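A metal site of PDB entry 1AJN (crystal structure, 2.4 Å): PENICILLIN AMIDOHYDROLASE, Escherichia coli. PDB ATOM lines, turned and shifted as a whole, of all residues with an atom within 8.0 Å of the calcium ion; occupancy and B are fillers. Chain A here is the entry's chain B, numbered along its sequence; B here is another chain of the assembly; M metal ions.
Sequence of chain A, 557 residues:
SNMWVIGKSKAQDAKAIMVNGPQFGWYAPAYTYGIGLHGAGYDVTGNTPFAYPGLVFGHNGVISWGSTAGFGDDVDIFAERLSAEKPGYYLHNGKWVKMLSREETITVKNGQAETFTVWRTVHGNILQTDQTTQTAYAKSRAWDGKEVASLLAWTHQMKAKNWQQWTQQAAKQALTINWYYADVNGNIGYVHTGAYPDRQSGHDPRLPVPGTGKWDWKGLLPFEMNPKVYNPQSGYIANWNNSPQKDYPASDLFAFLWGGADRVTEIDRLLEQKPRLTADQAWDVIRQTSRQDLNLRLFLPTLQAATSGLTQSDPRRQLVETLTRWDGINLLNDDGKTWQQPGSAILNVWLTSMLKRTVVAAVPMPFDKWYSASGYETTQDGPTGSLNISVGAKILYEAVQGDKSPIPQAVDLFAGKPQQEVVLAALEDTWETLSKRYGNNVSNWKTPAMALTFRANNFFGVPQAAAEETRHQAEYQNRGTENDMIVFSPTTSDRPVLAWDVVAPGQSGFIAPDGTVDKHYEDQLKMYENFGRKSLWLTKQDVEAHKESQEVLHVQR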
ATOM      1  N   GLY A  72     -30.352  22.407   7.097  1.00  0.00           N
ATOM      2  CA  GLY A  72     -31.290  21.520   7.809  1.00  0.00           C
ATOM      3  C   GLY A  72     -30.383  20.638   8.660  1.00  0.00           C
ATOM      4  O   GLY A  72     -29.182  20.656   8.407  1.00  0.00           O
ATOM      5  N   ASP A  73     -30.934  19.849   9.567  1.00  0.00           N
ATOM      6  CA  ASP A  73     -30.137  18.917  10.355  1.00  0.00           C
ATOM      7  C   ASP A  73     -30.117  17.553   9.651  1.00  0.00           C
ATOM      8  O   ASP A  73     -31.022  16.681   9.725  1.00  0.00           O
ATOM      9  CB  ASP A  73     -30.650  18.814  11.809  1.00  0.00           C
ATOM     10  CG  ASP A  73     -29.805  17.897  12.656  1.00  0.00           C
ATOM     11  OD1 ASP A  73     -29.014  17.119  12.075  1.00  0.00           O
ATOM     12  OD2 ASP A  73     -29.717  17.802  13.898  1.00  0.00           O
ATOM     13  N   ASP A  74     -28.978  17.259   9.006  1.00  0.00           N
ATOM     14  CA  ASP A  74     -28.881  15.985   8.296  1.00  0.00           C
ATOM     15  C   ASP A  74     -27.707  15.179   8.762  1.00  0.00           C
ATOM     16  O   ASP A  74     -27.205  14.325   8.029  1.00  0.00           O
ATOM     17  CB  ASP A  74     -28.798  16.194   6.790  1.00  0.00           C
ATOM     18  CG  ASP A  74     -27.665  17.107   6.381  1.00  0.00           C
ATOM     19  OD1 ASP A  74     -26.837  17.542   7.197  1.00  0.00           O
ATOM     20  OD2 ASP A  74     -27.528  17.443   5.215  1.00  0.00           O
ATOM     21  N   VAL A  75     -27.131  15.565   9.888  1.00  0.00           N
ATOM     22  CA  VAL A  75     -25.986  14.879  10.433  1.00  0.00           C
ATOM     23  C   VAL A  75     -26.231  14.640  11.925  1.00  0.00           C
ATOM     24  O   VAL A  75     -26.395  15.666  12.591  1.00  0.00           O
ATOM     25  CB  VAL A  75     -24.726  15.751  10.289  1.00  0.00           C
ATOM     26  CG1 VAL A  75     -23.514  15.177  11.029  1.00  0.00           C
ATOM     27  CG2 VAL A  75     -24.283  15.915   8.846  1.00  0.00           C
ATOM     28  N   ASP A  76     -26.162  13.414  12.435  1.00  0.00           N
ATOM     29  CA  ASP A  76     -26.234  13.152  13.856  1.00  0.00           C
ATOM     30  C   ASP A  76     -25.018  12.319  14.237  1.00  0.00           C
ATOM     31  O   ASP A  76     -24.450  11.537  13.447  1.00  0.00           O
ATOM     32  CB  ASP A  76     -27.460  12.376  14.307  1.00  0.00           C
ATOM     33  CG  ASP A  76     -28.780  12.981  13.964  1.00  0.00           C
ATOM     34  OD1 ASP A  76     -28.950  14.225  13.899  1.00  0.00           O
ATOM     35  OD2 ASP A  76     -29.721  12.183  13.766  1.00  0.00           O
ATOM     36  N   ILE A  77     -24.643  12.416  15.495  1.00  0.00           N
ATOM     37  CA  ILE A  77     -23.489  11.699  16.038  1.00  0.00           C
ATOM     38  C   ILE A  77     -23.918  10.493  16.860  1.00  0.00           C
ATOM     39  O   ILE A  77     -24.840  10.561  17.677  1.00  0.00           O
ATOM     40  CB  ILE A  77     -22.717  12.648  16.957  1.00  0.00           C
ATOM     41  CG1 ILE A  77     -22.277  13.900  16.208  1.00  0.00           C
ATOM     42  CG2 ILE A  77     -21.563  11.973  17.668  1.00  0.00           C
ATOM     43  CD1 ILE A  77     -21.197  13.697  15.201  1.00  0.00           C
ATOM     44  N   SER A 140     -22.661  10.518  11.403  1.00  0.00           N
ATOM     45  CA  SER A 140     -23.504   9.881  10.422  1.00  0.00           C
ATOM     46  C   SER A 140     -24.280  10.914   9.621  1.00  0.00           C
ATOM     47  O   SER A 140     -25.002  11.733  10.166  1.00  0.00           O
ATOM     48  CB  SER A 140     -24.299   8.833  11.192  1.00  0.00           C
ATOM     49  OG  SER A 140     -25.491   8.551  10.547  1.00  0.00           O
ATOM     50  N   PRO A 197     -32.985  12.138   7.867  1.00  0.00           N
ATOM     51  CA  PRO A 197     -33.216  10.903   8.584  1.00  0.00           C
ATOM     52  C   PRO A 197     -34.599  10.730   9.149  1.00  0.00           C
ATOM     53  O   PRO A 197     -35.274  11.702   9.422  1.00  0.00           O
ATOM     54  CB  PRO A 197     -32.151  10.824   9.708  1.00  0.00           C
ATOM     55  CG  PRO A 197     -31.766  12.276   9.862  1.00  0.00           C
ATOM     56  CD  PRO A 197     -32.046  13.015   8.589  1.00  0.00           C
ATOM     57  N   ARG A 199     -36.170   9.636  12.219  1.00  0.00           N
ATOM     58  CA  ARG A 199     -35.609   9.293  13.522  1.00  0.00           C
ATOM     59  C   ARG A 199     -36.624   8.561  14.401  1.00  0.00           C
ATOM     60  O   ARG A 199     -37.828   8.774  14.282  1.00  0.00           O
ATOM     61  CB  ARG A 199     -35.077  10.583  14.163  1.00  0.00           C
ATOM     62  CG  ARG A 199     -33.990  11.296  13.342  1.00  0.00           C
ATOM     63  CD  ARG A 199     -33.591  12.598  14.028  1.00  0.00           C
ATOM     64  NE  ARG A 199     -32.332  13.203  13.608  1.00  0.00           N
ATOM     65  CZ  ARG A 199     -32.436  14.243  12.745  1.00  0.00           C
ATOM     66  NH1 ARG A 199     -33.575  14.703  12.284  1.00  0.00           N
ATOM     67  NH2 ARG A 199     -31.316  14.820  12.355  1.00  0.00           N
ATOM     68  N   HIS A 203     -35.800  10.818  20.008  1.00  0.00           N
ATOM     69  CA  HIS A 203     -34.435  11.170  19.598  1.00  0.00           C
ATOM     70  C   HIS A 203     -34.369  12.699  19.552  1.00  0.00           C
ATOM     71  O   HIS A 203     -35.123  13.283  18.791  1.00  0.00           O
ATOM     72  CB  HIS A 203     -34.172  10.581  18.191  1.00  0.00           C
ATOM     73  CG  HIS A 203     -32.828  10.892  17.604  1.00  0.00           C
ATOM     74  ND1 HIS A 203     -32.182   9.971  16.782  1.00  0.00           N
ATOM     75  CD2 HIS A 203     -31.989  11.952  17.666  1.00  0.00           C
ATOM     76  CE1 HIS A 203     -31.017  10.421  16.365  1.00  0.00           C
ATOM     77  NE2 HIS A 203     -30.896  11.627  16.902  1.00  0.00           N
ATOM     78  N   ASP A 204     -33.602  13.353  20.367  1.00  0.00           N
ATOM     79  CA  ASP A 204     -33.453  14.812  20.327  1.00  0.00           C
ATOM     80  C   ASP A 204     -32.264  15.038  19.392  1.00  0.00           C
ATOM     81  O   ASP A 204     -31.131  14.588  19.675  1.00  0.00           O
ATOM     82  CB  ASP A 204     -33.148  15.317  21.731  1.00  0.00           C
ATOM     83  CG  ASP A 204     -32.858  16.811  21.857  1.00  0.00           C
ATOM     84  OD1 ASP A 204     -32.425  17.457  20.871  1.00  0.00           O
ATOM     85  OD2 ASP A 204     -33.154  17.360  22.947  1.00  0.00           O
ATOM     86  N   PRO A 205     -32.482  15.589  18.219  1.00  0.00           N
ATOM     87  CA  PRO A 205     -31.463  15.705  17.185  1.00  0.00           C
ATOM     88  C   PRO A 205     -30.372  16.721  17.470  1.00  0.00           C
ATOM     89  O   PRO A 205     -29.402  16.823  16.688  1.00  0.00           O
ATOM     90  CB  PRO A 205     -32.226  16.000  15.871  1.00  0.00           C
ATOM     91  CG  PRO A 205     -33.401  16.737  16.462  1.00  0.00           C
ATOM     92  CD  PRO A 205     -33.797  16.064  17.772  1.00  0.00           C
ATOM     93  N   ARG A 206     -30.307  17.366  18.636  1.00  0.00           N
ATOM     94  CA  ARG A 206     -29.258  18.316  18.970  1.00  0.00           C
ATOM     95  C   ARG A 206     -28.145  17.688  19.751  1.00  0.00           C
ATOM     96  O   ARG A 206     -27.117  18.319  20.046  1.00  0.00           O
ATOM     97  CB  ARG A 206     -29.750  19.504  19.790  1.00  0.00           C
ATOM     98  CG  ARG A 206     -31.011  20.159  19.156  1.00  0.00           C
ATOM     99  CD  ARG A 206     -31.692  21.017  20.211  1.00  0.00           C
ATOM    100  NE  ARG A 206     -32.334  20.243  21.273  1.00  0.00           N
ATOM    101  CZ  ARG A 206     -33.088  20.771  22.240  1.00  0.00           C
ATOM    102  NH1 ARG A 206     -33.258  22.098  22.239  1.00  0.00           N
ATOM    103  NH2 ARG A 206     -33.657  19.997  23.174  1.00  0.00           N
ATOM    104  N   LEU A 207     -28.379  16.430  20.137  1.00  0.00           N
ATOM    105  CA  LEU A 207     -27.371  15.788  21.019  1.00  0.00           C
ATOM    106  C   LEU A 207     -27.074  14.403  20.526  1.00  0.00           C
ATOM    107  O   LEU A 207     -27.914  13.768  19.932  1.00  0.00           O
ATOM    108  CB  LEU A 207     -27.978  15.788  22.426  1.00  0.00           C
ATOM    109  CG  LEU A 207     -28.376  17.121  23.091  1.00  0.00           C
ATOM    110  CD1 LEU A 207     -29.550  16.950  24.015  1.00  0.00           C
ATOM    111  CD2 LEU A 207     -27.147  17.696  23.775  1.00  0.00           C
ATOM    112  N   PRO A 208     -26.002  13.790  20.937  1.00  0.00           N
ATOM    113  CA  PRO A 208     -25.623  12.451  20.528  1.00  0.00           C
ATOM    114  C   PRO A 208     -26.563  11.348  20.930  1.00  0.00           C
ATOM    115  O   PRO A 208     -27.380  11.523  21.823  1.00  0.00           O
ATOM    116  CB  PRO A 208     -24.223  12.171  21.128  1.00  0.00           C
ATOM    117  CG  PRO A 208     -23.715  13.573  21.318  1.00  0.00           C
ATOM    118  CD  PRO A 208     -24.913  14.491  21.593  1.00  0.00           C
ATOM    119  N   TRP A 217     -31.421   5.249  12.954  1.00  0.00           N
ATOM    120  CA  TRP A 217     -32.450   5.836  12.104  1.00  0.00           C
ATOM    121  C   TRP A 217     -33.229   4.659  11.493  1.00  0.00           C
ATOM    122  O   TRP A 217     -32.771   3.526  11.369  1.00  0.00           O
ATOM    123  CB  TRP A 217     -31.893   6.684  10.984  1.00  0.00           C
ATOM    124  CG  TRP A 217     -31.022   7.835  11.329  1.00  0.00           C
ATOM    125  CD1 TRP A 217     -31.071   8.579  12.488  1.00  0.00           C
ATOM    126  CD2 TRP A 217     -30.017   8.433  10.505  1.00  0.00           C
ATOM    127  NE1 TRP A 217     -30.148   9.570  12.417  1.00  0.00           N
ATOM    128  CE2 TRP A 217     -29.489   9.525  11.240  1.00  0.00           C
ATOM    129  CE3 TRP A 217     -29.539   8.155   9.212  1.00  0.00           C
ATOM    130  CZ2 TRP A 217     -28.507  10.359  10.722  1.00  0.00           C
ATOM    131  CZ3 TRP A 217     -28.520   8.989   8.738  1.00  0.00           C
ATOM    132  CH2 TRP A 217     -28.008  10.075   9.460  1.00  0.00           C
ATOM    133  N   ALA A 250     -33.684  23.535  12.423  1.00  0.00           N
ATOM    134  CA  ALA A 250     -32.428  23.922  11.832  1.00  0.00           C
ATOM    135  C   ALA A 250     -31.311  22.989  12.237  1.00  0.00           C
ATOM    136  O   ALA A 250     -31.440  22.147  13.141  1.00  0.00           O
ATOM    137  CB  ALA A 250     -32.031  25.281  12.433  1.00  0.00           C
ATOM    138  N   SER A 251     -30.192  23.157  11.558  1.00  0.00           N
ATOM    139  CA  SER A 251     -28.942  22.466  11.877  1.00  0.00           C
ATOM    140  C   SER A 251     -28.827  22.425  13.419  1.00  0.00           C
ATOM    141  O   SER A 251     -29.147  23.428  14.031  1.00  0.00           O
ATOM    142  CB  SER A 251     -27.819  23.414  11.459  1.00  0.00           C
ATOM    143  OG  SER A 251     -26.528  22.888  11.672  1.00  0.00           O
ATOM    144  N   ASP A 252     -28.158  21.461  13.988  1.00  0.00           N
ATOM    145  CA  ASP A 252     -27.839  21.431  15.398  1.00  0.00           C
ATOM    146  C   ASP A 252     -26.658  22.287  15.837  1.00  0.00           C
ATOM    147  O   ASP A 252     -26.276  22.258  17.023  1.00  0.00           O
ATOM    148  CB  ASP A 252     -27.623  19.998  15.884  1.00  0.00           C
ATOM    149  CG  ASP A 252     -26.460  19.275  15.266  1.00  0.00           C
ATOM    150  OD1 ASP A 252     -25.314  19.816  15.269  1.00  0.00           O
ATOM    151  OD2 ASP A 252     -26.680  18.112  14.797  1.00  0.00           O
ATOM    152  N   LEU A 253     -26.083  23.136  14.964  1.00  0.00           N
ATOM    153  CA  LEU A 253     -24.951  23.949  15.375  1.00  0.00           C
ATOM    154  C   LEU A 253     -25.366  24.890  16.519  1.00  0.00           C
ATOM    155  O   LEU A 253     -26.287  25.687  16.322  1.00  0.00           O
ATOM    156  CB  LEU A 253     -24.425  24.830  14.245  1.00  0.00           C
ATOM    157  CG  LEU A 253     -23.719  24.116  13.108  1.00  0.00           C
ATOM    158  CD1 LEU A 253     -23.704  25.047  11.905  1.00  0.00           C
ATOM    159  CD2 LEU A 253     -22.325  23.693  13.545  1.00  0.00           C
ATOM    160  N   SER B 149     -22.492  20.108   8.675  1.00  0.00           N
ATOM    161  CA  SER B 149     -22.335  20.814   9.941  1.00  0.00           C
ATOM    162  C   SER B 149     -22.925  20.106  11.148  1.00  0.00           C
ATOM    163  O   SER B 149     -24.148  19.882  11.094  1.00  0.00           O
ATOM    164  CB  SER B 149     -23.181  22.105   9.787  1.00  0.00           C
ATOM    165  OG  SER B 149     -22.651  23.005   8.859  1.00  0.00           O
ATOM    166  N   THR B 150     -22.219  19.927  12.249  1.00  0.00           N
ATOM    167  CA  THR B 150     -22.851  19.424  13.459  1.00  0.00           C
ATOM    168  C   THR B 150     -22.035  19.965  14.639  1.00  0.00           C
ATOM    169  O   THR B 150     -20.830  20.033  14.470  1.00  0.00           O
ATOM    170  CB  THR B 150     -22.931  17.890  13.525  1.00  0.00           C
ATOM    171  OG1 THR B 150     -23.695  17.440  14.636  1.00  0.00           O
ATOM    172  CG2 THR B 150     -21.556  17.265  13.721  1.00  0.00           C
ATOM    173  N   SER B 151     -22.613  20.122  15.829  1.00  0.00           N
ATOM    174  CA  SER B 151     -21.776  20.474  16.989  1.00  0.00           C
ATOM    175  C   SER B 151     -22.334  19.654  18.174  1.00  0.00           C
ATOM    176  O   SER B 151     -22.070  20.063  19.293  1.00  0.00           O
ATOM    177  CB  SER B 151     -21.741  21.975  17.339  1.00  0.00           C
ATOM    178  OG  SER B 151     -23.092  22.423  17.664  1.00  0.00           O
ATOM    179  N   GLU B 152     -22.866  18.465  17.862  1.00  0.00           N
ATOM    180  CA  GLU B 152     -23.587  17.666  18.827  1.00  0.00           C
ATOM    181  C   GLU B 152     -22.772  17.358  20.073  1.00  0.00           C
ATOM    182  O   GLU B 152     -23.242  17.393  21.217  1.00  0.00           O
ATOM    183  CB  GLU B 152     -24.220  16.395  18.278  1.00  0.00           C
ATOM    184  CG  GLU B 152     -25.501  16.613  17.495  1.00  0.00           C
ATOM    185  CD  GLU B 152     -26.108  15.313  16.967  1.00  0.00           C
ATOM    186  OE1 GLU B 152     -25.694  14.242  17.468  1.00  0.00           O
ATOM    187  OE2 GLU B 152     -26.979  15.387  16.048  1.00  0.00           O
ATOM    188  N   ASN B 155     -22.589  20.579  22.009  1.00  0.00           N
ATOM    189  CA  ASN B 155     -23.851  20.814  22.661  1.00  0.00           C
ATOM    190  C   ASN B 155     -23.971  20.013  23.967  1.00  0.00           C
ATOM    191  O   ASN B 155     -24.486  20.565  24.948  1.00  0.00           O
ATOM    192  CB  ASN B 155     -25.030  20.491  21.764  1.00  0.00           C
ATOM    193  CG  ASN B 155     -25.031  21.286  20.464  1.00  0.00           C
ATOM    194  OD1 ASN B 155     -24.214  22.179  20.257  1.00  0.00           O
ATOM    195  ND2 ASN B 155     -25.953  20.860  19.607  1.00  0.00           N
HETATM  196 CA    CA M   1     -28.064  16.374  14.516  1.00  0.00          CA
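The side-chain hydroxyl of Thr 150 of chain B sits at hydrogen-bond distance from the side-chain carboxylate of Asp 252 (2.9 Å).
The backbone NH (N) of Ile 77 lies within hydrogen-bond range of the side-chain carboxylate (OE1) of Glu 152 of chain B.
O of Asp 76 is in hydrogen-bond range of N of Ser 140 (2.9 Å).
The guanidinium group (NE) of Arg 199 lies within salt-bridge range of the side-chain carboxylate (OD2) of Asp 76, 2.8 Å away.
OD1 of Asp 252 sits at hydrogen-bond distance from N of Ser 151 of chain B, 2.8 Å away.
The side-chain carboxylate of Asp 76 lies within hydrogen-bond range of the indole nitrogen of Trp 217, 3.0 Å away.
OD2 of Asp 76 sits at hydrogen-bond distance from NE2 of His 203.
The backbone NH (N) of Glu 152 of chain B lies close to the side-chain hydroxyl (OG1) of Thr 150 of chain B, 3.5 Å away.
The nearest printed residue that does not touch the calcium ion is Arg 199 (4.2 Å).
The calcium ion is bound by the side-chain carboxylate (OE2) of Glu 152 of chain B, the side-chain carboxylate (OD2) of Asp 252, the side-chain carboxylate (OD2) of Asp 73, the side-chain carboxylate (OD1) of Asp 76, the backbone carbonyl oxygen (O) of Pro 205, the backbone carbonyl oxygen (O) of Val 75 and the side-chain carboxylate (OD1) of Asp 73.
The calcium ion has seven donor atoms within binding distance.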
